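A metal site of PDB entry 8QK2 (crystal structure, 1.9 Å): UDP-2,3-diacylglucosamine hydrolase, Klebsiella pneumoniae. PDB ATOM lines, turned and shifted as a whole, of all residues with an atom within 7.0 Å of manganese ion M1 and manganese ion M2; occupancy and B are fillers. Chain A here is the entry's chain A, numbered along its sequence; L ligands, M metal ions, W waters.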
ATOM      1  N   ALA A   7      14.820   0.102  -0.907  1.00  0.00           N
ATOM      2  CA  ALA A   7      14.705  -0.114  -2.342  1.00  0.00           C
ATOM      3  C   ALA A   7      16.081   0.013  -3.004  1.00  0.00           C
ATOM      4  O   ALA A   7      17.040   0.448  -2.355  1.00  0.00           O
ATOM      5  CB  ALA A   7      13.701   0.855  -2.928  1.00  0.00           C
ATOM      6  N   ASP A   8      16.155  -0.386  -4.284  1.00  0.00           N
ATOM      7  CA  ASP A   8      17.300  -0.084  -5.119  1.00  0.00           C
ATOM      8  C   ASP A   8      18.599  -0.680  -4.549  1.00  0.00           C
ATOM      9  O   ASP A   8      19.659  -0.055  -4.647  1.00  0.00           O
ATOM     10  CB  ASP A   8      17.426   1.425  -5.375  1.00  0.00           C
ATOM     11  CG  ASP A   8      16.206   1.996  -6.062  1.00  0.00           C
ATOM     12  OD1 ASP A   8      15.971   1.647  -7.223  1.00  0.00           O
ATOM     13  OD2 ASP A   8      15.459   2.761  -5.424  1.00  0.00           O
ATOM     14  N   LEU A   9      18.511  -1.926  -4.076  1.00  0.00           N
ATOM     15  CA  LEU A   9      19.687  -2.686  -3.664  1.00  0.00           C
ATOM     16  C   LEU A   9      20.502  -3.167  -4.864  1.00  0.00           C
ATOM     17  O   LEU A   9      21.719  -3.304  -4.775  1.00  0.00           O
ATOM     18  CB  LEU A   9      19.240  -3.862  -2.799  1.00  0.00           C
ATOM     19  CG  LEU A   9      18.681  -3.442  -1.427  1.00  0.00           C
ATOM     20  CD1 LEU A   9      17.175  -3.222  -1.467  1.00  0.00           C
ATOM     21  CD2 LEU A   9      19.032  -4.472  -0.386  1.00  0.00           C
ATOM     22  N   HIS A  10      19.834  -3.419  -5.997  1.00  0.00           N
ATOM     23  CA  HIS A  10      20.502  -3.851  -7.222  1.00  0.00           C
ATOM     24  C   HIS A  10      21.449  -5.026  -6.961  1.00  0.00           C
ATOM     25  O   HIS A  10      22.578  -5.027  -7.432  1.00  0.00           O
ATOM     26  CB  HIS A  10      21.171  -2.651  -7.904  1.00  0.00           C
ATOM     27  CG  HIS A  10      20.179  -1.668  -8.426  1.00  0.00           C
ATOM     28  ND1 HIS A  10      19.813  -1.683  -9.759  1.00  0.00           N
ATOM     29  CD2 HIS A  10      19.465  -0.704  -7.858  1.00  0.00           C
ATOM     30  CE1 HIS A  10      18.899  -0.745  -9.967  1.00  0.00           C
ATOM     31  NE2 HIS A  10      18.679  -0.141  -8.826  1.00  0.00           N
ATOM     32  N   LEU A  39      10.709  -1.746  -2.052  1.00  0.00           N
ATOM     33  CA  LEU A  39      10.018  -0.998  -3.071  1.00  0.00           C
ATOM     34  C   LEU A  39      10.764  -1.081  -4.399  1.00  0.00           C
ATOM     35  O   LEU A  39      10.938  -0.080  -5.096  1.00  0.00           O
ATOM     36  CB  LEU A  39       9.872   0.440  -2.562  1.00  0.00           C
ATOM     37  CG  LEU A  39       9.137   0.603  -1.231  1.00  0.00           C
ATOM     38  CD1 LEU A  39       8.761   2.068  -1.009  1.00  0.00           C
ATOM     39  CD2 LEU A  39       7.890  -0.277  -1.166  1.00  0.00           C
ATOM     40  N   GLY A  40      11.205  -2.296  -4.748  1.00  0.00           N
ATOM     41  CA  GLY A  40      11.640  -2.593  -6.099  1.00  0.00           C
ATOM     42  C   GLY A  40      13.145  -2.442  -6.284  1.00  0.00           C
ATOM     43  O   GLY A  40      13.805  -1.826  -5.444  1.00  0.00           O
ATOM     44  N   ASP A  41      13.646  -3.015  -7.386  1.00  0.00           N
ATOM     45  CA  ASP A  41      15.065  -3.085  -7.709  1.00  0.00           C
ATOM     46  C   ASP A  41      15.823  -3.702  -6.536  1.00  0.00           C
ATOM     47  O   ASP A  41      16.900  -3.243  -6.166  1.00  0.00           O
ATOM     48  CB  ASP A  41      15.610  -1.690  -8.080  1.00  0.00           C
ATOM     49  CG  ASP A  41      15.135  -1.147  -9.426  1.00  0.00           C
ATOM     50  OD1 ASP A  41      14.390  -1.881 -10.134  1.00  0.00           O
ATOM     51  OD2 ASP A  41      15.513   0.035  -9.727  1.00  0.00           O
ATOM     52  N   GLU A  44      19.446  -6.553  -9.542  1.00  0.00           N
ATOM     53  CA  GLU A  44      19.936  -5.814 -10.692  1.00  0.00           C
ATOM     54  C   GLU A  44      19.274  -6.297 -11.979  1.00  0.00           C
ATOM     55  O   GLU A  44      19.192  -5.534 -12.949  1.00  0.00           O
ATOM     56  CB  GLU A  44      21.458  -5.977 -10.811  1.00  0.00           C
ATOM     57  CG  GLU A  44      22.078  -5.348 -12.052  1.00  0.00           C
ATOM     58  CD  GLU A  44      21.842  -3.864 -12.251  1.00  0.00           C
ATOM     59  OE1 GLU A  44      21.432  -3.168 -11.285  1.00  0.00           O
ATOM     60  OE2 GLU A  44      22.051  -3.391 -13.387  1.00  0.00           O
ATOM     61  N   GLY A  78      10.404  -3.311  -9.194  1.00  0.00           N
ATOM     62  CA  GLY A  78      11.076  -2.225  -9.897  1.00  0.00           C
ATOM     63  C   GLY A  78      11.088  -2.446 -11.412  1.00  0.00           C
ATOM     64  O   GLY A  78      10.468  -3.369 -11.917  1.00  0.00           O
ATOM     65  N   ASN A  79      11.791  -1.569 -12.128  1.00  0.00           N
ATOM     66  CA  ASN A  79      11.992  -1.734 -13.554  1.00  0.00           C
ATOM     67  C   ASN A  79      12.947  -2.891 -13.829  1.00  0.00           C
ATOM     68  O   ASN A  79      12.925  -3.481 -14.919  1.00  0.00           O
ATOM     69  CB  ASN A  79      12.510  -0.467 -14.249  1.00  0.00           C
ATOM     70  CG  ASN A  79      13.717   0.111 -13.556  1.00  0.00           C
ATOM     71  OD1 ASN A  79      13.638   0.361 -12.360  1.00  0.00           O
ATOM     72  ND2 ASN A  79      14.821   0.309 -14.254  1.00  0.00           N
ATOM     73  N   ARG A  80      13.834  -3.180 -12.869  1.00  0.00           N
ATOM     74  CA  ARG A  80      14.884  -4.159 -13.092  1.00  0.00           C
ATOM     75  C   ARG A  80      14.338  -5.566 -12.843  1.00  0.00           C
ATOM     76  O   ARG A  80      14.772  -6.491 -13.524  1.00  0.00           O
ATOM     77  CB  ARG A  80      16.095  -3.910 -12.185  1.00  0.00           C
ATOM     78  CG  ARG A  80      16.815  -2.584 -12.411  1.00  0.00           C
ATOM     79  CD  ARG A  80      17.308  -2.339 -13.820  1.00  0.00           C
ATOM     80  NE  ARG A  80      18.288  -3.310 -14.295  1.00  0.00           N
ATOM     81  CZ  ARG A  80      18.857  -3.286 -15.498  1.00  0.00           C
ATOM     82  NH1 ARG A  80      18.613  -2.294 -16.348  1.00  0.00           N
ATOM     83  NH2 ARG A  80      19.694  -4.239 -15.845  1.00  0.00           N
ATOM     84  N   HIS A 114       7.486   1.984  -6.589  1.00  0.00           N
ATOM     85  CA  HIS A 114       8.883   2.017  -7.013  1.00  0.00           C
ATOM     86  C   HIS A 114       9.309   3.443  -7.377  1.00  0.00           C
ATOM     87  O   HIS A 114      10.373   3.888  -6.946  1.00  0.00           O
ATOM     88  CB  HIS A 114       9.193   1.056  -8.161  1.00  0.00           C
ATOM     89  CG  HIS A 114      10.647   0.993  -8.472  1.00  0.00           C
ATOM     90  ND1 HIS A 114      11.594   0.647  -7.521  1.00  0.00           N
ATOM     91  CD2 HIS A 114      11.337   1.311  -9.587  1.00  0.00           C
ATOM     92  CE1 HIS A 114      12.792   0.716  -8.079  1.00  0.00           C
ATOM     93  NE2 HIS A 114      12.659   1.107  -9.339  1.00  0.00           N
ATOM     94  N   GLY A 115       8.491   4.114  -8.202  1.00  0.00           N
ATOM     95  CA  GLY A 115       8.729   5.500  -8.583  1.00  0.00           C
ATOM     96  C   GLY A 115       8.943   5.668 -10.075  1.00  0.00           C
ATOM     97  O   GLY A 115       8.813   6.780 -10.603  1.00  0.00           O
ATOM     98  N   ASP A 116       9.225   4.572 -10.791  1.00  0.00           N
ATOM     99  CA  ASP A 116       9.456   4.635 -12.226  1.00  0.00           C
ATOM    100  C   ASP A 116       8.221   5.152 -12.968  1.00  0.00           C
ATOM    101  O   ASP A 116       8.371   5.844 -13.985  1.00  0.00           O
ATOM    102  CB  ASP A 116       9.939   3.286 -12.773  1.00  0.00           C
ATOM    103  CG  ASP A 116       8.928   2.163 -12.616  1.00  0.00           C
ATOM    104  OD1 ASP A 116       8.546   1.854 -11.454  1.00  0.00           O
ATOM    105  OD2 ASP A 116       8.498   1.607 -13.661  1.00  0.00           O
ATOM    106  N   TYR A 125      11.593   4.911 -21.795  1.00  0.00           N
ATOM    107  CA  TYR A 125      11.380   3.996 -20.694  1.00  0.00           C
ATOM    108  C   TYR A 125       9.914   3.529 -20.675  1.00  0.00           C
ATOM    109  O   TYR A 125       9.650   2.326 -20.555  1.00  0.00           O
ATOM    110  CB  TYR A 125      11.743   4.584 -19.329  1.00  0.00           C
ATOM    111  CG  TYR A 125      11.335   3.626 -18.253  1.00  0.00           C
ATOM    112  CD1 TYR A 125      11.900   2.368 -18.198  1.00  0.00           C
ATOM    113  CD2 TYR A 125      10.273   3.896 -17.400  1.00  0.00           C
ATOM    114  CE1 TYR A 125      11.470   1.420 -17.283  1.00  0.00           C
ATOM    115  CE2 TYR A 125       9.838   2.966 -16.472  1.00  0.00           C
ATOM    116  CZ  TYR A 125      10.433   1.718 -16.428  1.00  0.00           C
ATOM    117  OH  TYR A 125      10.003   0.764 -15.536  1.00  0.00           O
ATOM    118  N   ILE A 171      19.399   7.899 -14.600  1.00  0.00           N
ATOM    119  CA  ILE A 171      17.991   7.573 -14.483  1.00  0.00           C
ATOM    120  C   ILE A 171      17.210   8.893 -14.427  1.00  0.00           C
ATOM    121  O   ILE A 171      17.494   9.739 -13.599  1.00  0.00           O
ATOM    122  CB  ILE A 171      17.761   6.667 -13.246  1.00  0.00           C
ATOM    123  CG1 ILE A 171      18.493   5.325 -13.414  1.00  0.00           C
ATOM    124  CG2 ILE A 171      16.281   6.469 -12.973  1.00  0.00           C
ATOM    125  CD1 ILE A 171      18.396   4.416 -12.212  1.00  0.00           C
ATOM    126  N   GLY A 194      11.546   4.913  -4.520  1.00  0.00           N
ATOM    127  CA  GLY A 194      12.949   4.866  -4.910  1.00  0.00           C
ATOM    128  C   GLY A 194      13.100   5.186  -6.392  1.00  0.00           C
ATOM    129  O   GLY A 194      12.586   6.200  -6.871  1.00  0.00           O
ATOM    130  N   HIS A 195      13.809   4.298  -7.107  1.00  0.00           N
ATOM    131  CA  HIS A 195      14.015   4.347  -8.547  1.00  0.00           C
ATOM    132  C   HIS A 195      15.028   5.423  -8.986  1.00  0.00           C
ATOM    133  O   HIS A 195      15.897   5.131  -9.806  1.00  0.00           O
ATOM    134  CB  HIS A 195      12.700   4.497  -9.332  1.00  0.00           C
ATOM    135  CG  HIS A 195      12.953   4.486 -10.797  1.00  0.00           C
ATOM    136  ND1 HIS A 195      13.540   3.431 -11.456  1.00  0.00           N
ATOM    137  CD2 HIS A 195      12.765   5.445 -11.709  1.00  0.00           C
ATOM    138  CE1 HIS A 195      13.661   3.747 -12.741  1.00  0.00           C
ATOM    139  NE2 HIS A 195      13.191   4.955 -12.920  1.00  0.00           N
ATOM    140  N   THR A 196      14.855   6.659  -8.512  1.00  0.00           N
ATOM    141  CA  THR A 196      15.583   7.802  -9.040  1.00  0.00           C
ATOM    142  C   THR A 196      17.007   7.871  -8.474  1.00  0.00           C
ATOM    143  O   THR A 196      17.812   8.642  -8.984  1.00  0.00           O
ATOM    144  CB  THR A 196      14.850   9.128  -8.782  1.00  0.00           C
ATOM    145  OG1 THR A 196      14.742   9.383  -7.377  1.00  0.00           O
ATOM    146  CG2 THR A 196      13.464   9.178  -9.384  1.00  0.00           C
ATOM    147  N   HIS A 197      17.280   7.101  -7.405  1.00  0.00           N
ATOM    148  CA  HIS A 197      18.596   7.057  -6.765  1.00  0.00           C
ATOM    149  C   HIS A 197      19.037   8.446  -6.281  1.00  0.00           C
ATOM    150  O   HIS A 197      20.226   8.703  -6.224  1.00  0.00           O
ATOM    151  CB  HIS A 197      19.655   6.429  -7.694  1.00  0.00           C
ATOM    152  CG  HIS A 197      19.375   5.017  -8.129  1.00  0.00           C
ATOM    153  ND1 HIS A 197      20.234   4.283  -8.918  1.00  0.00           N
ATOM    154  CD2 HIS A 197      18.341   4.207  -7.845  1.00  0.00           C
ATOM    155  CE1 HIS A 197      19.710   3.090  -9.135  1.00  0.00           C
ATOM    156  NE2 HIS A 197      18.558   3.014  -8.497  1.00  0.00           N
ATOM    157  N   ALA A 218      19.979   4.268  -3.583  1.00  0.00           N
ATOM    158  CA  ALA A 218      20.532   2.999  -4.007  1.00  0.00           C
ATOM    159  C   ALA A 218      21.610   2.546  -3.034  1.00  0.00           C
ATOM    160  O   ALA A 218      22.244   3.349  -2.344  1.00  0.00           O
ATOM    161  CB  ALA A 218      21.068   3.125  -5.415  1.00  0.00           C
HETATM  162  C1  LIG L   1      10.592  -9.454 -21.346  1.00  0.00           C
HETATM  163  C2  LIG L   1      10.840  -9.540 -22.694  1.00  0.00           C
HETATM  164  N1  LIG L   1      13.917  -8.902 -20.056  1.00  0.00           N
HETATM  165  C3  LIG L   1      13.668  -9.363 -18.717  1.00  0.00           C
HETATM  166  C4  LIG L   1      14.478  -8.457 -17.797  1.00  0.00           C
HETATM  167  C5  LIG L   1      15.247  -9.228 -20.484  1.00  0.00           C
HETATM  168  C6  LIG L   1      16.204  -8.355 -19.631  1.00  0.00           C
HETATM  169  C7  LIG L   1      12.148  -9.393 -23.159  1.00  0.00           C
HETATM  170  N2  LIG L   1      13.151  -9.217 -22.286  1.00  0.00           N
HETATM  171  C8  LIG L   1      12.907  -9.231 -20.962  1.00  0.00           C
HETATM  172  N3  LIG L   1      11.636  -9.280 -20.503  1.00  0.00           N
HETATM  173  N4  LIG L   1      15.923  -8.563 -18.146  1.00  0.00           N
HETATM  174  S1  LIG L   1      16.829  -7.534 -17.192  1.00  0.00           S
HETATM  175  C9  LIG L   1      16.527  -5.850 -17.626  1.00  0.00           C
HETATM  176  O1  LIG L   1      16.492  -7.782 -15.810  1.00  0.00           O
HETATM  177  O2  LIG L   1      18.183  -7.840 -17.428  1.00  0.00           O
HETATM  178  C10 LIG L   1      17.210  -5.313 -18.672  1.00  0.00           C
HETATM  179  C11 LIG L   1      16.984  -4.009 -19.061  1.00  0.00           C
HETATM  180  C12 LIG L   1      16.084  -3.195 -18.381  1.00  0.00           C
HETATM  181  C13 LIG L   1      15.586  -5.051 -16.901  1.00  0.00           C
HETATM  182  C14 LIG L   1      15.368  -3.714 -17.301  1.00  0.00           C
HETATM  183  N5  LIG L   1      15.874  -1.906 -18.893  1.00  0.00           N
HETATM  184  C15 LIG L   1      15.269  -0.867 -18.217  1.00  0.00           C
HETATM  185  O3  LIG L   1      14.878  -0.996 -17.066  1.00  0.00           O
HETATM  186  C16 LIG L   1      15.132   0.461 -18.952  1.00  0.00           C
HETATM  187  C17 LIG L   1      14.686   0.464 -20.266  1.00  0.00           C
HETATM  188  C18 LIG L   1      14.586   1.669 -20.957  1.00  0.00           C
HETATM  189  C19 LIG L   1      14.970   2.855 -20.360  1.00  0.00           C
HETATM  190  C20 LIG L   1      15.440   2.857 -19.051  1.00  0.00           C
HETATM  191  C21 LIG L   1      15.552   1.654 -18.344  1.00  0.00           C
HETATM  192  N6  LIG L   1      15.993   1.662 -16.953  1.00  0.00           N
HETATM  193  C22 LIG L   1      15.679   2.950 -16.295  1.00  0.00           C
HETATM  194  S2  LIG L   1      17.590   1.342 -16.838  1.00  0.00           S
HETATM  195  C23 LIG L   1      18.530   2.756 -17.379  1.00  0.00           C
HETATM  196  O4  LIG L   1      17.908   1.025 -15.477  1.00  0.00           O
HETATM  197  O5  LIG L   1      17.900   0.231 -17.647  1.00  0.00           O
HETATM  198  C24 LIG L   1       9.182  -9.572 -20.786  1.00  0.00           C
HETATM  199  C25 LIG L   1      12.425  -9.475 -24.542  1.00  0.00           C
HETATM  200  N7  LIG L   1      12.786  -9.523 -25.616  1.00  0.00           N
HETATM  201 MN    MN M   1      17.127   1.390  -8.937  1.00  0.00          MN
HETATM  202 MN    MN M   2      14.362   1.512 -10.728  1.00  0.00          MN
HETATM  203  O   HOH W   1      16.227   2.590 -10.442  1.00  0.00           O
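The side-chain amide nitrogen (ND2) of Asn 79 sits at hydrogen-bond distance from an oxygen (O3) of the ligand.
O5 of the ligand sits at hydrogen-bond distance from NH1 of Arg 80, at 2.9 Å.
OD2 of Asp 8 is in hydrogen-bond range of N of His 195, 2.8 Å away.
The backbone carbonyl oxygen (O) of Gly 40 lies within hydrogen-bond range of the backbone NH (N) of Asp 8 (3.0 Å).
The side-chain carboxylate (OD1) of Asp 41 lies within hydrogen-bond range of the backbone NH (N) of Arg 80 (3.1 Å).
O of Asp 41 lies within hydrogen-bond range of N of Leu 9 (2.9 Å).
A ring nitrogen (ND1) of His 10 sits at hydrogen-bond distance from the side-chain carboxylate (OE1) of Glu 44.
N of Gly 194 sits at hydrogen-bond distance from O of His 114, at 2.9 Å.
A ring nitrogen (ND1) of His 114 sits at hydrogen-bond distance from the backbone carbonyl oxygen of Leu 39, at 2.6 Å.
Four residues have an atom within 4 Å of manganese ion M1: Asp 8, His 10, Asp 41 and His 197.
Along chain A the residues within 4 Å of manganese ion M1 span positions 8 to 197.
Of the 21 residues printed, 5 come within 4 Å of manganese ion M2.
Manganese ion M1 is bound by the side-chain carboxylate of Asp 8 (2.1 Å), water W1 (2.1 Å), a ring nitrogen (NE2) of His 10 (2.2 Å), a ring nitrogen (NE2) of His 197 (2.2 Å) and the side-chain carboxylate of Asp 41 (2.3 Å).
Manganese ion M1 has five donor atoms within binding distance.
Manganese ion M2 is bound by the side-chain carboxylate (OD2) of Asp 41 (2.1 Å), the side-chain amide oxygen (OD1) of Asn 79 (2.1 Å), water W1 (2.2 Å), a ring nitrogen (ND1) of His 195 (2.2 Å) and a ring nitrogen (NE2) of His 114 (2.2 Å).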
